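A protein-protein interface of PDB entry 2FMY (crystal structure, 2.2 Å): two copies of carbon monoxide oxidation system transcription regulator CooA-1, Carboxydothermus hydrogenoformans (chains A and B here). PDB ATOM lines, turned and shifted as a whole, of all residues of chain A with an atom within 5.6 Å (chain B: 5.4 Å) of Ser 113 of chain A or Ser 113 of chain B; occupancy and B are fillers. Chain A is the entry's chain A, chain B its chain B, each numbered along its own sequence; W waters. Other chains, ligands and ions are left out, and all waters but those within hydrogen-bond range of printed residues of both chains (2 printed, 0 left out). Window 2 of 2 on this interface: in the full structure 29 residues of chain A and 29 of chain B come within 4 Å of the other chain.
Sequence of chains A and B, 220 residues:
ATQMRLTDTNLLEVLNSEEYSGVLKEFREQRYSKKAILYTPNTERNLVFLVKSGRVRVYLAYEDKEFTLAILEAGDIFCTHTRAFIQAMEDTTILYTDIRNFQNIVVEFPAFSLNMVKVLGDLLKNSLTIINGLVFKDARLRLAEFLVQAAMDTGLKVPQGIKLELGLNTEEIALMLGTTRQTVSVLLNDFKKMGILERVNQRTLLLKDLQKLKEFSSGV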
ATOM      1  N   VAL A 106     -14.075 -28.912   0.284  1.00  0.00           N
ATOM      2  CA  VAL A 106     -13.868 -27.470   0.409  1.00  0.00           C
ATOM      3  C   VAL A 106     -12.374 -27.069   0.441  1.00  0.00           C
ATOM      4  O   VAL A 106     -11.999 -25.997  -0.022  1.00  0.00           O
ATOM      5  CB  VAL A 106     -14.679 -26.864   1.600  1.00  0.00           C
ATOM      6  CG1 VAL A 106     -13.969 -27.085   2.951  1.00  0.00           C
ATOM      7  CG2 VAL A 106     -14.968 -25.376   1.342  1.00  0.00           C
ATOM      8  N   PHE A 109     -10.902 -28.152  -3.646  1.00  0.00           N
ATOM      9  CA  PHE A 109     -11.606 -27.667  -4.824  1.00  0.00           C
ATOM     10  C   PHE A 109     -12.110 -26.246  -4.563  1.00  0.00           C
ATOM     11  O   PHE A 109     -13.180 -26.069  -3.979  1.00  0.00           O
ATOM     12  CB  PHE A 109     -12.747 -28.633  -5.189  1.00  0.00           C
ATOM     13  CG  PHE A 109     -12.271 -30.028  -5.547  1.00  0.00           C
ATOM     14  CD1 PHE A 109     -11.786 -30.307  -6.817  1.00  0.00           C
ATOM     15  CD2 PHE A 109     -12.291 -31.050  -4.603  1.00  0.00           C
ATOM     16  CE1 PHE A 109     -11.333 -31.588  -7.158  1.00  0.00           C
ATOM     17  CE2 PHE A 109     -11.843 -32.336  -4.927  1.00  0.00           C
ATOM     18  CZ  PHE A 109     -11.367 -32.606  -6.214  1.00  0.00           C
ATOM     19  N   PRO A 110     -11.324 -25.227  -4.987  1.00  0.00           N
ATOM     20  CA  PRO A 110     -11.498 -23.816  -4.579  1.00  0.00           C
ATOM     21  C   PRO A 110     -12.827 -23.150  -4.938  1.00  0.00           C
ATOM     22  O   PRO A 110     -13.211 -22.190  -4.280  1.00  0.00           O
ATOM     23  CB  PRO A 110     -10.355 -23.095  -5.303  1.00  0.00           C
ATOM     24  CG  PRO A 110      -9.358 -24.173  -5.620  1.00  0.00           C
ATOM     25  CD  PRO A 110     -10.190 -25.375  -5.916  1.00  0.00           C
ATOM     26  N   ALA A 111     -13.516 -23.629  -5.969  1.00  0.00           N
ATOM     27  CA  ALA A 111     -14.789 -23.025  -6.365  1.00  0.00           C
ATOM     28  C   ALA A 111     -15.842 -23.055  -5.261  1.00  0.00           C
ATOM     29  O   ALA A 111     -16.692 -22.166  -5.192  1.00  0.00           O
ATOM     30  CB  ALA A 111     -15.331 -23.680  -7.630  1.00  0.00           C
ATOM     31  N   PHE A 112     -15.800 -24.081  -4.411  1.00  0.00           N
ATOM     32  CA  PHE A 112     -16.795 -24.218  -3.342  1.00  0.00           C
ATOM     33  C   PHE A 112     -16.688 -23.076  -2.332  1.00  0.00           C
ATOM     34  O   PHE A 112     -17.686 -22.455  -2.010  1.00  0.00           O
ATOM     35  CB  PHE A 112     -16.718 -25.583  -2.642  1.00  0.00           C
ATOM     36  CG  PHE A 112     -17.259 -26.729  -3.471  1.00  0.00           C
ATOM     37  CD1 PHE A 112     -16.420 -27.449  -4.316  1.00  0.00           C
ATOM     38  CD2 PHE A 112     -18.604 -27.086  -3.401  1.00  0.00           C
ATOM     39  CE1 PHE A 112     -16.918 -28.505  -5.088  1.00  0.00           C
ATOM     40  CE2 PHE A 112     -19.114 -28.156  -4.164  1.00  0.00           C
ATOM     41  CZ  PHE A 112     -18.259 -28.865  -5.005  1.00  0.00           C
ATOM     42  N   SER A 113     -15.488 -22.786  -1.844  1.00  0.00           N
ATOM     43  CA  SER A 113     -15.354 -21.719  -0.854  1.00  0.00           C
ATOM     44  C   SER A 113     -15.656 -20.335  -1.446  1.00  0.00           C
ATOM     45  O   SER A 113     -16.142 -19.456  -0.737  1.00  0.00           O
ATOM     46  CB  SER A 113     -13.980 -21.742  -0.190  1.00  0.00           C
ATOM     47  OG  SER A 113     -12.981 -21.472  -1.146  1.00  0.00           O
ATOM     48  N   LEU A 114     -15.385 -20.143  -2.741  1.00  0.00           N
ATOM     49  CA  LEU A 114     -15.720 -18.873  -3.392  1.00  0.00           C
ATOM     50  C   LEU A 114     -17.234 -18.649  -3.448  1.00  0.00           C
ATOM     51  O   LEU A 114     -17.691 -17.514  -3.292  1.00  0.00           O
ATOM     52  CB  LEU A 114     -15.104 -18.753  -4.800  1.00  0.00           C
ATOM     53  CG  LEU A 114     -13.579 -18.655  -4.891  1.00  0.00           C
ATOM     54  CD1 LEU A 114     -13.120 -18.696  -6.345  1.00  0.00           C
ATOM     55  CD2 LEU A 114     -13.035 -17.411  -4.161  1.00  0.00           C
ATOM     56  N   ASN A 115     -17.998 -19.724  -3.671  1.00  0.00           N
ATOM     57  CA  ASN A 115     -19.457 -19.639  -3.679  1.00  0.00           C
ATOM     58  C   ASN A 115     -19.997 -19.414  -2.280  1.00  0.00           C
ATOM     59  O   ASN A 115     -20.972 -18.699  -2.103  1.00  0.00           O
ATOM     60  CB  ASN A 115     -20.129 -20.888  -4.272  1.00  0.00           C
ATOM     61  CG  ASN A 115     -21.656 -20.832  -4.132  1.00  0.00           C
ATOM     62  OD1 ASN A 115     -22.222 -21.338  -3.160  1.00  0.00           O
ATOM     63  ND2 ASN A 115     -22.314 -20.149  -5.065  1.00  0.00           N
ATOM     64  N   MET A 116     -19.350 -20.040  -1.299  1.00  0.00           N
ATOM     65  CA  MET A 116     -19.705 -19.865   0.095  1.00  0.00           C
ATOM     66  C   MET A 116     -19.561 -18.417   0.556  1.00  0.00           C
ATOM     67  O   MET A 116     -20.430 -17.904   1.264  1.00  0.00           O
ATOM     68  CB  MET A 116     -18.882 -20.819   0.960  1.00  0.00           C
ATOM     69  CG  MET A 116     -19.380 -22.254   0.901  1.00  0.00           C
ATOM     70  SD  MET A 116     -18.206 -23.398   1.648  1.00  0.00           S
ATOM     71  CE  MET A 116     -18.388 -23.003   3.380  1.00  0.00           C
ATOM     72  N   VAL A 117     -18.486 -17.761   0.125  1.00  0.00           N
ATOM     73  CA  VAL A 117     -18.237 -16.335   0.400  1.00  0.00           C
ATOM     74  C   VAL A 117     -19.374 -15.442  -0.124  1.00  0.00           C
ATOM     75  O   VAL A 117     -19.859 -14.567   0.588  1.00  0.00           O
ATOM     76  CB  VAL A 117     -16.872 -15.897  -0.206  1.00  0.00           C
ATOM     77  CG1 VAL A 117     -16.800 -14.401  -0.380  1.00  0.00           C
ATOM     78  CG2 VAL A 117     -15.702 -16.423   0.644  1.00  0.00           C
ATOM     79  N   LYS A 118     -19.779 -15.673  -1.375  1.00  0.00           N
ATOM     80  CA  LYS A 118     -20.926 -15.003  -2.015  1.00  0.00           C
ATOM     81  C   LYS A 118     -22.244 -15.201  -1.238  1.00  0.00           C
ATOM     82  O   LYS A 118     -22.954 -14.234  -0.935  1.00  0.00           O
ATOM     83  CB  LYS A 118     -21.072 -15.509  -3.456  1.00  0.00           C
ATOM     84  CG  LYS A 118     -22.252 -14.944  -4.224  1.00  0.00           C
ATOM     85  CD  LYS A 118     -22.404 -15.611  -5.592  1.00  0.00           C
ATOM     86  CE  LYS A 118     -23.123 -16.960  -5.494  1.00  0.00           C
ATOM     87  NZ  LYS A 118     -24.601 -16.825  -5.273  1.00  0.00           N
ATOM     88  N   VAL B 106      -7.317 -13.587  -4.001  1.00  0.00           N
ATOM     89  CA  VAL B 106      -8.380 -14.412  -3.424  1.00  0.00           C
ATOM     90  C   VAL B 106      -8.836 -15.539  -4.370  1.00  0.00           C
ATOM     91  O   VAL B 106      -9.251 -16.607  -3.922  1.00  0.00           O
ATOM     92  CB  VAL B 106      -9.571 -13.546  -2.898  1.00  0.00           C
ATOM     93  CG1 VAL B 106     -10.554 -13.193  -4.013  1.00  0.00           C
ATOM     94  CG2 VAL B 106     -10.276 -14.249  -1.753  1.00  0.00           C
ATOM     95  N   PHE B 109      -4.955 -17.673  -4.694  1.00  0.00           N
ATOM     96  CA  PHE B 109      -4.403 -18.309  -3.501  1.00  0.00           C
ATOM     97  C   PHE B 109      -5.525 -18.758  -2.550  1.00  0.00           C
ATOM     98  O   PHE B 109      -6.057 -17.953  -1.785  1.00  0.00           O
ATOM     99  CB  PHE B 109      -3.380 -17.384  -2.827  1.00  0.00           C
ATOM    100  CG  PHE B 109      -2.167 -17.108  -3.685  1.00  0.00           C
ATOM    101  CD1 PHE B 109      -1.028 -17.900  -3.577  1.00  0.00           C
ATOM    102  CD2 PHE B 109      -2.176 -16.074  -4.620  1.00  0.00           C
ATOM    103  CE1 PHE B 109       0.090 -17.661  -4.378  1.00  0.00           C
ATOM    104  CE2 PHE B 109      -1.068 -15.828  -5.430  1.00  0.00           C
ATOM    105  CZ  PHE B 109       0.069 -16.622  -5.305  1.00  0.00           C
ATOM    106  N   PRO B 110      -5.886 -20.057  -2.623  1.00  0.00           N
ATOM    107  CA  PRO B 110      -7.051 -20.692  -1.978  1.00  0.00           C
ATOM    108  C   PRO B 110      -7.216 -20.462  -0.474  1.00  0.00           C
ATOM    109  O   PRO B 110      -8.345 -20.441   0.010  1.00  0.00           O
ATOM    110  CB  PRO B 110      -6.861 -22.192  -2.276  1.00  0.00           C
ATOM    111  CG  PRO B 110      -5.444 -22.335  -2.806  1.00  0.00           C
ATOM    112  CD  PRO B 110      -5.110 -21.020  -3.429  1.00  0.00           C
ATOM    113  N   ALA B 111      -6.118 -20.274   0.252  1.00  0.00           N
ATOM    114  CA  ALA B 111      -6.159 -20.119   1.710  1.00  0.00           C
ATOM    115  C   ALA B 111      -6.924 -18.892   2.183  1.00  0.00           C
ATOM    116  O   ALA B 111      -7.371 -18.833   3.338  1.00  0.00           O
ATOM    117  CB  ALA B 111      -4.748 -20.110   2.286  1.00  0.00           C
ATOM    118  N   PHE B 112      -7.077 -17.912   1.296  1.00  0.00           N
ATOM    119  CA  PHE B 112      -7.751 -16.675   1.653  1.00  0.00           C
ATOM    120  C   PHE B 112      -9.267 -16.815   1.758  1.00  0.00           C
ATOM    121  O   PHE B 112      -9.864 -16.382   2.749  1.00  0.00           O
ATOM    122  CB  PHE B 112      -7.333 -15.548   0.706  1.00  0.00           C
ATOM    123  CG  PHE B 112      -5.930 -15.051   0.952  1.00  0.00           C
ATOM    124  CD1 PHE B 112      -5.672 -14.137   1.971  1.00  0.00           C
ATOM    125  CD2 PHE B 112      -4.875 -15.497   0.177  1.00  0.00           C
ATOM    126  CE1 PHE B 112      -4.376 -13.675   2.213  1.00  0.00           C
ATOM    127  CE2 PHE B 112      -3.570 -15.036   0.407  1.00  0.00           C
ATOM    128  CZ  PHE B 112      -3.329 -14.125   1.425  1.00  0.00           C
ATOM    129  N   SER B 113      -9.882 -17.434   0.758  1.00  0.00           N
ATOM    130  CA  SER B 113     -11.334 -17.671   0.777  1.00  0.00           C
ATOM    131  C   SER B 113     -11.755 -18.608   1.917  1.00  0.00           C
ATOM    132  O   SER B 113     -12.822 -18.425   2.502  1.00  0.00           O
ATOM    133  CB  SER B 113     -11.826 -18.191  -0.568  1.00  0.00           C
ATOM    134  OG  SER B 113     -11.182 -19.401  -0.888  1.00  0.00           O
ATOM    135  N   LEU B 114     -10.900 -19.579   2.244  1.00  0.00           N
ATOM    136  CA  LEU B 114     -11.088 -20.440   3.426  1.00  0.00           C
ATOM    137  C   LEU B 114     -11.189 -19.664   4.745  1.00  0.00           C
ATOM    138  O   LEU B 114     -12.060 -19.958   5.565  1.00  0.00           O
ATOM    139  CB  LEU B 114      -9.983 -21.507   3.522  1.00  0.00           C
ATOM    140  CG  LEU B 114     -10.044 -22.636   2.498  1.00  0.00           C
ATOM    141  CD1 LEU B 114      -8.852 -23.592   2.663  1.00  0.00           C
ATOM    142  CD2 LEU B 114     -11.384 -23.380   2.600  1.00  0.00           C
ATOM    143  N   ASN B 115     -10.316 -18.675   4.941  1.00  0.00           N
ATOM    144  CA  ASN B 115     -10.413 -17.775   6.106  1.00  0.00           C
ATOM    145  C   ASN B 115     -11.613 -16.805   6.070  1.00  0.00           C
ATOM    146  O   ASN B 115     -12.263 -16.558   7.102  1.00  0.00           O
ATOM    147  CB  ASN B 115      -9.117 -16.992   6.316  1.00  0.00           C
ATOM    148  CG  ASN B 115      -9.161 -16.135   7.572  1.00  0.00           C
ATOM    149  OD1 ASN B 115      -9.397 -14.937   7.497  1.00  0.00           O
ATOM    150  ND2 ASN B 115      -8.979 -16.762   8.735  1.00  0.00           N
ATOM    151  N   MET B 116     -11.909 -16.260   4.891  1.00  0.00           N
ATOM    152  CA  MET B 116     -13.107 -15.437   4.702  1.00  0.00           C
ATOM    153  C   MET B 116     -14.372 -16.212   5.108  1.00  0.00           C
ATOM    154  O   MET B 116     -15.242 -15.677   5.782  1.00  0.00           O
ATOM    155  CB  MET B 116     -13.233 -14.998   3.242  1.00  0.00           C
ATOM    156  CG  MET B 116     -12.164 -14.021   2.762  1.00  0.00           C
ATOM    157  SD  MET B 116     -12.439 -13.503   1.057  1.00  0.00           S
ATOM    158  CE  MET B 116     -13.997 -12.642   1.199  1.00  0.00           C
ATOM    159  N   VAL B 117     -14.460 -17.474   4.686  1.00  0.00           N
ATOM    160  CA  VAL B 117     -15.590 -18.336   5.028  1.00  0.00           C
ATOM    161  C   VAL B 117     -15.724 -18.446   6.556  1.00  0.00           C
ATOM    162  O   VAL B 117     -16.821 -18.334   7.087  1.00  0.00           O
ATOM    163  CB  VAL B 117     -15.492 -19.731   4.339  1.00  0.00           C
ATOM    164  CG1 VAL B 117     -16.458 -20.732   4.965  1.00  0.00           C
ATOM    165  CG2 VAL B 117     -15.765 -19.621   2.831  1.00  0.00           C
ATOM    166  N   LYS B 118     -14.597 -18.633   7.240  1.00  0.00           N
ATOM    167  CA  LYS B 118     -14.539 -18.723   8.704  1.00  0.00           C
ATOM    168  C   LYS B 118     -14.986 -17.428   9.389  1.00  0.00           C
ATOM    169  O   LYS B 118     -15.714 -17.459  10.389  1.00  0.00           O
ATOM    170  CB  LYS B 118     -13.124 -19.121   9.135  1.00  0.00           C
ATOM    171  CG  LYS B 118     -12.695 -18.675  10.528  1.00  0.00           C
ATOM    172  CD  LYS B 118     -11.329 -19.234  10.870  1.00  0.00           C
ATOM    173  CE  LYS B 118     -10.521 -18.307  11.780  1.00  0.00           C
ATOM    174  NZ  LYS B 118     -11.334 -17.397  12.652  1.00  0.00           N
HETATM  175  O   HOH W   1     -11.358 -20.634  -3.302  1.00  0.00           O
HETATM  176  O   HOH W   2     -10.303 -22.421  -1.129  1.00  0.00           O
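Hydrophobic or aromatic side chains of chain B that line the printed part of chain A: Leu 114, Met 116 and Val 117. Of the 11 printed residues of chain A, 5 touch a printed residue of chain B. Hydrophobic or aromatic side chains of chain A within 4 Å of the printed part of chain B: Leu 114, Met 116 and Val 117. Along chain A the printed residues that touch a printed residue of chain B span positions 106 to 117. Among the printed residues, 9 pairs touch across the chains. Among the printed residues, no Asp or Glu carboxylate lies within 4 Å of a Lys or Arg side-chain nitrogen of the other chain.
The backbone carbonyl oxygen (O) of Pro 110 of chain B is in hydrogen-bond range of the side-chain hydroxyl (OG) of Ser 113 of chain B, 3.2 Å away. The backbone carbonyl oxygen (O) of Pro 110 of chain A is in hydrogen-bond range of the side-chain hydroxyl (OG) of Ser 113 of chain A (3.2 Å).
CD2 of Leu 114 of chain B touches O of Val 106 of chain A, 3.8 Å away. Ser 113 of chain A touches Val 117 of chain B (O to CG2, 3.6 Å). CD2 of Leu 114 of chain A touches O of Val 106 of chain B, 3.9 Å away. Leu 114 of chain A touches Ser 113 of chain B. CG1 of Val 117 of chain B touches CE of Met 116 of chain A, 3.4 Å away. Val 117 of chain A touches Ser 113 of chain B (CG2 to O, 3.97 Å). Val 117 of chain A touches Met 116 of chain B. CG2 of Val 117 of chain B touches CG2 of Val 117 of chain A, at 3.9 Å.
Val 106 of chain A touches Leu 114 of chain B, and with the chains exchanged Leu 114 of chain A touches Val 106 of chain B. Ser 113 of chain A touches its own counterpart, Ser 113 of chain B. Ser 113 of chain A touches Val 117 of chain B, and with the chains exchanged Val 117 of chain A touches Ser 113 of chain B. Met 116 of chain A touches Val 117 of chain B, and with the chains exchanged Val 117 of chain A touches Met 116 of chain B. Positions printed for both chains: 106, 109, 110, 111, 112, 113, 114, 115, 116, 117 and 118.
The side-chain hydroxyl (OG) of Ser 113 of chain B lies within hydrogen-bond range of the side-chain hydroxyl (OG) of Ser 113 of chain A (2.8 Å).
Water W1 lies within hydrogen-bond range of O of Pro 110 of chain A (2.6 Å), OG of Ser 113 of chain B (2.7 Å) and OG of Ser 113 of chain A (2.8 Å). Water W2 lies within hydrogen-bond range of the side-chain hydroxyl (OG) of Ser 113 of chain A (2.8 Å), the backbone carbonyl oxygen (O) of Pro 110 of chain B (3.0 Å) and the side-chain hydroxyl (OG) of Ser 113 of chain B (3.2 Å).
Ser 113 of chain A touches just these residues of chain B: Ser 113 (2.8 Å) and Val 117 (3.6 Å). Of chain A, only Ser 113 (2.8 Å), Leu 114 (3.9 Å) and Val 117 (3.97 Å) come within 4 Å of Ser 113 of chain B. Printed residues of chain A within 4 Å of Leu 114 of chain B: Val 106 (3.8 Å). Printed residues of chain A within 4 Å of Val 106 of chain B: Leu 114. Of the printed residues of chain B, Met 116 of chain A touches Val 117 (3.4 Å). The nearest residue of chain A that does not touch Ser 113 of chain B is Pro 110 of chain A (4.8 Å). The nearest printed residue of chain A that does not touch Met 116 of chain B is Leu 114 of chain A (6.5 Å).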
